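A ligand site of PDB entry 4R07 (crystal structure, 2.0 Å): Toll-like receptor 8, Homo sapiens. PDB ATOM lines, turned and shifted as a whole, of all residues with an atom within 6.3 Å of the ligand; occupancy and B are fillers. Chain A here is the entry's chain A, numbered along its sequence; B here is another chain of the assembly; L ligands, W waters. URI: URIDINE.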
ATOM      1  N   ALA A 496      18.706 -29.573  -5.095  1.00  0.00           N
ATOM      2  CA  ALA A 496      18.613 -28.629  -3.992  1.00  0.00           C
ATOM      3  C   ALA A 496      17.773 -27.399  -4.303  1.00  0.00           C
ATOM      4  O   ALA A 496      17.788 -26.422  -3.523  1.00  0.00           O
ATOM      5  CB  ALA A 496      20.024 -28.192  -3.618  1.00  0.00           C
ATOM      6  N   VAL A 498      14.755 -24.619  -5.469  1.00  0.00           N
ATOM      7  CA  VAL A 498      13.439 -24.117  -5.142  1.00  0.00           C
ATOM      8  C   VAL A 498      12.592 -24.235  -6.391  1.00  0.00           C
ATOM      9  O   VAL A 498      12.747 -23.484  -7.356  1.00  0.00           O
ATOM     10  CB  VAL A 498      13.493 -22.620  -4.724  1.00  0.00           C
ATOM     11  CG1 VAL A 498      12.094 -22.101  -4.455  1.00  0.00           C
ATOM     12  CG2 VAL A 498      14.391 -22.420  -3.500  1.00  0.00           C
ATOM     13  N   ASP A 521      14.549 -27.517  -1.661  1.00  0.00           N
ATOM     14  CA  ASP A 521      14.322 -26.336  -0.833  1.00  0.00           C
ATOM     15  C   ASP A 521      12.919 -25.770  -1.049  1.00  0.00           C
ATOM     16  O   ASP A 521      12.610 -25.178  -2.095  1.00  0.00           O
ATOM     17  CB  ASP A 521      15.352 -25.289  -1.170  1.00  0.00           C
ATOM     18  CG  ASP A 521      15.323 -24.104  -0.224  1.00  0.00           C
ATOM     19  OD1 ASP A 521      14.746 -24.226   0.859  1.00  0.00           O
ATOM     20  OD2 ASP A 521      16.000 -23.099  -0.541  1.00  0.00           O
ATOM     21  N   ASP A 523      10.839 -23.322  -0.782  1.00  0.00           N
ATOM     22  CA  ASP A 523      10.638 -21.898  -0.522  1.00  0.00           C
ATOM     23  C   ASP A 523       9.609 -21.210  -1.436  1.00  0.00           C
ATOM     24  O   ASP A 523       9.559 -20.007  -1.455  1.00  0.00           O
ATOM     25  CB  ASP A 523      11.953 -21.145  -0.599  1.00  0.00           C
ATOM     26  CG  ASP A 523      11.812 -19.664  -0.172  1.00  0.00           C
ATOM     27  OD1 ASP A 523      11.141 -19.351   0.819  1.00  0.00           O
ATOM     28  OD2 ASP A 523      12.368 -18.807  -0.857  1.00  0.00           O
ATOM     29  N   GLY A 550      16.066 -22.612  10.562  1.00  0.00           N
ATOM     30  CA  GLY A 550      16.155 -21.217  10.169  1.00  0.00           C
ATOM     31  C   GLY A 550      15.844 -20.891   8.720  1.00  0.00           C
ATOM     32  O   GLY A 550      15.870 -19.727   8.337  1.00  0.00           O
ATOM     33  N   VAL A 551      15.638 -21.907   7.888  1.00  0.00           N
ATOM     34  CA  VAL A 551      15.203 -21.616   6.514  1.00  0.00           C
ATOM     35  C   VAL A 551      13.740 -21.965   6.387  1.00  0.00           C
ATOM     36  O   VAL A 551      13.173 -22.614   7.270  1.00  0.00           O
ATOM     37  CB  VAL A 551      16.036 -22.389   5.467  1.00  0.00           C
ATOM     38  CG1 VAL A 551      17.511 -22.144   5.671  1.00  0.00           C
ATOM     39  CG2 VAL A 551      15.741 -23.886   5.549  1.00  0.00           C
ATOM     40  N   THR A 552      13.119 -21.511   5.311  1.00  0.00           N
ATOM     41  CA  THR A 552      11.675 -21.654   5.129  1.00  0.00           C
ATOM     42  C   THR A 552      11.363 -23.063   4.637  1.00  0.00           C
ATOM     43  O   THR A 552      12.149 -23.639   3.903  1.00  0.00           O
ATOM     44  CB  THR A 552      11.146 -20.669   4.108  1.00  0.00           C
ATOM     45  OG1 THR A 552      11.886 -20.786   2.888  1.00  0.00           O
ATOM     46  CG2 THR A 552      11.289 -19.216   4.618  1.00  0.00           C
ATOM     47  N   PHE B 239       8.974 -14.241  12.102  1.00  0.00           N
ATOM     48  CA  PHE B 239       8.853 -14.910  10.804  1.00  0.00           C
ATOM     49  C   PHE B 239       9.609 -16.250  10.865  1.00  0.00           C
ATOM     50  O   PHE B 239      10.797 -16.284  11.173  1.00  0.00           O
ATOM     51  CB  PHE B 239       9.364 -14.068   9.641  1.00  0.00           C
ATOM     52  CG  PHE B 239       9.326 -14.800   8.339  1.00  0.00           C
ATOM     53  CD1 PHE B 239       8.100 -15.085   7.743  1.00  0.00           C
ATOM     54  CD2 PHE B 239      10.484 -15.354   7.811  1.00  0.00           C
ATOM     55  CE1 PHE B 239       8.037 -15.893   6.611  1.00  0.00           C
ATOM     56  CE2 PHE B 239      10.425 -16.143   6.649  1.00  0.00           C
ATOM     57  CZ  PHE B 239       9.209 -16.416   6.046  1.00  0.00           C
ATOM     58  N   ASN B 240       8.900 -17.339  10.561  1.00  0.00           N
ATOM     59  CA  ASN B 240       9.473 -18.681  10.488  1.00  0.00           C
ATOM     60  C   ASN B 240       9.999 -19.202  11.806  1.00  0.00           C
ATOM     61  O   ASN B 240      10.910 -20.023  11.838  1.00  0.00           O
ATOM     62  CB  ASN B 240      10.618 -18.726   9.496  1.00  0.00           C
ATOM     63  CG  ASN B 240      10.922 -20.129   9.040  1.00  0.00           C
ATOM     64  OD1 ASN B 240      10.025 -20.970   8.938  1.00  0.00           O
ATOM     65  ND2 ASN B 240      12.187 -20.399   8.813  1.00  0.00           N
ATOM     66  N   PHE B 324      21.083 -14.501  10.735  1.00  0.00           N
ATOM     67  CA  PHE B 324      19.637 -14.513  10.521  1.00  0.00           C
ATOM     68  C   PHE B 324      18.994 -13.118  10.697  1.00  0.00           C
ATOM     69  O   PHE B 324      18.013 -12.940  11.417  1.00  0.00           O
ATOM     70  CB  PHE B 324      18.993 -15.562  11.396  1.00  0.00           C
ATOM     71  CG  PHE B 324      19.336 -16.966  10.952  1.00  0.00           C
ATOM     72  CD1 PHE B 324      18.789 -17.479   9.800  1.00  0.00           C
ATOM     73  CD2 PHE B 324      20.259 -17.734  11.662  1.00  0.00           C
ATOM     74  CE1 PHE B 324      19.139 -18.746   9.359  1.00  0.00           C
ATOM     75  CE2 PHE B 324      20.583 -19.017  11.244  1.00  0.00           C
ATOM     76  CZ  PHE B 324      20.063 -19.505  10.059  1.00  0.00           C
ATOM     77  N   TYR B 326      18.270 -11.789   7.666  1.00  0.00           N
ATOM     78  CA  TYR B 326      17.758 -11.670   6.298  1.00  0.00           C
ATOM     79  C   TYR B 326      16.411 -10.947   6.216  1.00  0.00           C
ATOM     80  O   TYR B 326      15.571 -11.063   7.107  1.00  0.00           O
ATOM     81  CB  TYR B 326      17.624 -13.061   5.612  1.00  0.00           C
ATOM     82  CG  TYR B 326      16.573 -13.971   6.197  1.00  0.00           C
ATOM     83  CD1 TYR B 326      16.889 -14.963   7.115  1.00  0.00           C
ATOM     84  CD2 TYR B 326      15.283 -13.898   5.772  1.00  0.00           C
ATOM     85  CE1 TYR B 326      15.948 -15.824   7.589  1.00  0.00           C
ATOM     86  CE2 TYR B 326      14.325 -14.752   6.261  1.00  0.00           C
ATOM     87  CZ  TYR B 326      14.658 -15.722   7.143  1.00  0.00           C
ATOM     88  OH  TYR B 326      13.678 -16.595   7.582  1.00  0.00           O
ATOM     89  N   ILE B 327      16.161 -10.305   5.085  1.00  0.00           N
ATOM     90  CA  ILE B 327      14.811  -9.828   4.749  1.00  0.00           C
ATOM     91  C   ILE B 327      14.115 -10.901   3.901  1.00  0.00           C
ATOM     92  O   ILE B 327      14.659 -11.321   2.856  1.00  0.00           O
ATOM     93  CB  ILE B 327      14.892  -8.528   3.931  1.00  0.00           C
ATOM     94  CG1 ILE B 327      15.629  -7.428   4.729  1.00  0.00           C
ATOM     95  CG2 ILE B 327      13.476  -8.104   3.509  1.00  0.00           C
ATOM     96  CD1 ILE B 327      16.416  -6.458   3.848  1.00  0.00           C
ATOM     97  N   LYS B 328      12.959 -11.362   4.348  1.00  0.00           N
ATOM     98  CA  LYS B 328      12.357 -12.492   3.689  1.00  0.00           C
ATOM     99  C   LYS B 328      11.981 -12.171   2.241  1.00  0.00           C
ATOM    100  O   LYS B 328      11.693 -11.008   1.890  1.00  0.00           O
ATOM    101  CB  LYS B 328      11.146 -13.038   4.434  1.00  0.00           C
ATOM    102  CG  LYS B 328      10.036 -12.044   4.601  1.00  0.00           C
ATOM    103  CD  LYS B 328       8.765 -12.748   5.061  1.00  0.00           C
ATOM    104  CE  LYS B 328       7.564 -11.885   4.724  1.00  0.00           C
ATOM    105  NZ  LYS B 328       6.305 -12.504   5.178  1.00  0.00           N
ATOM    106  N   GLY B 329      12.111 -13.202   1.392  1.00  0.00           N
ATOM    107  CA  GLY B 329      11.884 -13.091  -0.041  1.00  0.00           C
ATOM    108  C   GLY B 329      13.001 -12.372  -0.773  1.00  0.00           C
ATOM    109  O   GLY B 329      13.087 -12.459  -1.977  1.00  0.00           O
ATOM    110  N   SER B 330      13.893 -11.702  -0.032  1.00  0.00           N
ATOM    111  CA  SER B 330      14.985 -10.979  -0.625  1.00  0.00           C
ATOM    112  C   SER B 330      16.247 -11.831  -0.773  1.00  0.00           C
ATOM    113  O   SER B 330      16.743 -12.437   0.177  1.00  0.00           O
ATOM    114  CB  SER B 330      15.302  -9.788   0.256  1.00  0.00           C
ATOM    115  OG  SER B 330      16.197  -8.909  -0.390  1.00  0.00           O
ATOM    116  N   TYR B 331      16.839 -11.764  -1.956  1.00  0.00           N
ATOM    117  CA  TYR B 331      17.990 -12.553  -2.277  1.00  0.00           C
ATOM    118  C   TYR B 331      18.903 -11.693  -3.097  1.00  0.00           C
ATOM    119  O   TYR B 331      19.132 -11.969  -4.255  1.00  0.00           O
ATOM    120  CB  TYR B 331      17.554 -13.786  -3.061  1.00  0.00           C
ATOM    121  CG  TYR B 331      18.546 -14.913  -3.258  1.00  0.00           C
ATOM    122  CD1 TYR B 331      19.620 -15.178  -2.357  1.00  0.00           C
ATOM    123  CD2 TYR B 331      18.342 -15.810  -4.289  1.00  0.00           C
ATOM    124  CE1 TYR B 331      20.458 -16.301  -2.552  1.00  0.00           C
ATOM    125  CE2 TYR B 331      19.182 -16.901  -4.483  1.00  0.00           C
ATOM    126  CZ  TYR B 331      20.212 -17.158  -3.618  1.00  0.00           C
ATOM    127  OH  TYR B 331      20.969 -18.258  -3.945  1.00  0.00           O
ATOM    128  N   VAL B 356      21.712 -14.167   3.563  1.00  0.00           N
ATOM    129  CA  VAL B 356      21.068 -14.736   2.388  1.00  0.00           C
ATOM    130  C   VAL B 356      21.356 -13.901   1.151  1.00  0.00           C
ATOM    131  O   VAL B 356      20.716 -12.863   0.947  1.00  0.00           O
ATOM    132  CB  VAL B 356      19.545 -14.925   2.548  1.00  0.00           C
ATOM    133  CG1 VAL B 356      18.944 -15.491   1.271  1.00  0.00           C
ATOM    134  CG2 VAL B 356      19.203 -15.852   3.692  1.00  0.00           C
ATOM    135  N   ASN B 382      23.565 -19.236   3.739  1.00  0.00           N
ATOM    136  CA  ASN B 382      23.313 -17.966   3.033  1.00  0.00           C
ATOM    137  C   ASN B 382      22.877 -18.196   1.582  1.00  0.00           C
ATOM    138  O   ASN B 382      22.662 -17.249   0.854  1.00  0.00           O
ATOM    139  CB  ASN B 382      24.595 -17.112   3.040  1.00  0.00           C
ATOM    140  CG  ASN B 382      24.705 -16.264   4.293  1.00  0.00           C
ATOM    141  OD1 ASN B 382      23.810 -15.457   4.583  1.00  0.00           O
ATOM    142  ND2 ASN B 382      25.718 -16.548   5.131  1.00  0.00           N
ATOM    143  N   PHE B 383      22.783 -19.455   1.163  1.00  0.00           N
ATOM    144  CA  PHE B 383      22.358 -19.819  -0.180  1.00  0.00           C
ATOM    145  C   PHE B 383      23.258 -19.182  -1.206  1.00  0.00           C
ATOM    146  O   PHE B 383      22.848 -18.960  -2.340  1.00  0.00           O
ATOM    147  CB  PHE B 383      20.871 -19.473  -0.458  1.00  0.00           C
ATOM    148  CG  PHE B 383      19.909 -20.240   0.399  1.00  0.00           C
ATOM    149  CD1 PHE B 383      19.600 -21.560   0.120  1.00  0.00           C
ATOM    150  CD2 PHE B 383      19.292 -19.651   1.463  1.00  0.00           C
ATOM    151  CE1 PHE B 383      18.790 -22.283   0.943  1.00  0.00           C
ATOM    152  CE2 PHE B 383      18.438 -20.354   2.272  1.00  0.00           C
ATOM    153  CZ  PHE B 383      18.189 -21.679   2.012  1.00  0.00           C
ATOM    154  N   ARG B 407      25.148 -22.811  -1.765  1.00  0.00           N
ATOM    155  CA  ARG B 407      24.871 -23.344  -3.092  1.00  0.00           C
ATOM    156  C   ARG B 407      26.086 -23.283  -3.986  1.00  0.00           C
ATOM    157  O   ARG B 407      25.975 -23.120  -5.222  1.00  0.00           O
ATOM    158  CB  ARG B 407      23.727 -22.585  -3.781  1.00  0.00           C
ATOM    159  CG  ARG B 407      22.405 -22.600  -3.027  1.00  0.00           C
ATOM    160  CD  ARG B 407      21.282 -22.129  -3.910  1.00  0.00           C
ATOM    161  NE  ARG B 407      19.987 -22.397  -3.328  1.00  0.00           N
ATOM    162  CZ  ARG B 407      19.364 -23.552  -3.415  1.00  0.00           C
ATOM    163  NH1 ARG B 407      19.916 -24.532  -4.103  1.00  0.00           N
ATOM    164  NH2 ARG B 407      18.217 -23.731  -2.794  1.00  0.00           N
HETATM  165  N1  URI L   1      15.927 -18.199   0.174  1.00  0.00           N
HETATM  166  C2  URI L   1      15.764 -19.581   0.290  1.00  0.00           C
HETATM  167  N3  URI L   1      16.356 -20.411  -0.606  1.00  0.00           N
HETATM  168  C4  URI L   1      17.101 -19.954  -1.610  1.00  0.00           C
HETATM  169  C5  URI L   1      17.272 -18.592  -1.734  1.00  0.00           C
HETATM  170  C6  URI L   1      16.691 -17.736  -0.793  1.00  0.00           C
HETATM  171  O2  URI L   1      15.071 -19.983   1.290  1.00  0.00           O
HETATM  172  O4  URI L   1      17.634 -20.714  -2.482  1.00  0.00           O
HETATM  173  C1' URI L   1      15.402 -17.273   1.186  1.00  0.00           C
HETATM  174  C2' URI L   1      13.944 -17.358   1.557  1.00  0.00           C
HETATM  175  C3' URI L   1      13.857 -16.834   2.975  1.00  0.00           C
HETATM  176  C4' URI L   1      15.266 -17.074   3.533  1.00  0.00           C
HETATM  177  O2' URI L   1      13.220 -16.445   0.756  1.00  0.00           O
HETATM  178  O3' URI L   1      13.532 -15.422   2.898  1.00  0.00           O
HETATM  179  O4' URI L   1      16.071 -17.485   2.448  1.00  0.00           O
HETATM  180  C5' URI L   1      15.318 -18.227   4.522  1.00  0.00           C
HETATM  181  O5' URI L   1      14.928 -19.432   3.837  1.00  0.00           O
HETATM  182  O   HOH W   1      17.128 -20.607  -5.038  1.00  0.00           O
HETATM  183  O   HOH W   2      15.870 -13.790   2.049  1.00  0.00           O
HETATM  184  O   HOH W   3      14.222 -22.311   2.426  1.00  0.00           O
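The guanidinium group (NH2) of Arg 407 of chain B lies within salt-bridge range of the side-chain carboxylate (OD2) of Asp 521 (3.2 Å). The side-chain carboxylate of Asp 523 is in hydrogen-bond range of the side-chain hydroxyl of Thr 552, at 2.6 Å. The backbone carbonyl oxygen of Ala 496 sits at hydrogen-bond distance from the guanidinium group of Arg 407 of chain B (2.8 Å). The side-chain hydroxyl (OH) of Tyr 331 of chain B is in hydrogen-bond range of the backbone carbonyl oxygen (O) of Phe 383 of chain B (2.6 Å). The side-chain amide nitrogen (ND2) of Asn 240 of chain B sits at hydrogen-bond distance from the backbone carbonyl oxygen (O) of Val 551, at 2.9 Å. The backbone NH (N) of Val 356 of chain B sits at hydrogen-bond distance from the side-chain amide oxygen (OD1) of Asn 382 of chain B (2.7 Å).
Residues that only touch the ligand: Lys 328 of chain B, Phe 383 of chain B, Val 551, Tyr 326 of chain B, Val 356 of chain B, Tyr 331 of chain B and Val 498. Hydrophobic or aromatic side chains within 4 Å of the ligand: Val 498, Val 551, Tyr 326 of chain B, Tyr 331 of chain B, Val 356 of chain B and Phe 383 of chain B. Within 4 Å of the ligand: Val 498, Asp 521, Asp 523, Val 551, Thr 552, Tyr 326 of chain B, Lys 328 of chain B, Gly 329 of chain B, Tyr 331 of chain B, Val 356 of chain B, Phe 383 of chain B and Arg 407 of chain B.
Water W3 lies within hydrogen-bond range of the side-chain carboxylate (OD1) of Asp 521 (2.5 Å), an oxygen (O2) of the ligand (2.7 Å) and the side-chain hydroxyl (OG1) of Thr 552 (2.8 Å). Water W2 lies within hydrogen-bond range of the backbone carbonyl oxygen (O) of Ser 330 of chain B (2.5 Å) and an oxygen (O3') of the ligand (3.0 Å).
OD2 of Asp 521 sits at hydrogen-bond distance from N3 of the ligand, 2.7 Å away. An oxygen (O2') of the ligand lies within hydrogen-bond range of the side-chain carboxylate (OD2) of Asp 523, 3.0 Å away. NE of Arg 407 of chain B is in hydrogen-bond range of O4 of the ligand (3.0 Å). N of Gly 329 of chain B lies within hydrogen-bond range of O3' of the ligand (3.0 Å). N of Thr 552 is in hydrogen-bond range of O5' of the ligand, 3.1 Å away. An oxygen (O5') of the ligand lies within hydrogen-bond range of the side-chain hydroxyl (OG1) of Thr 552 (3.5 Å).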
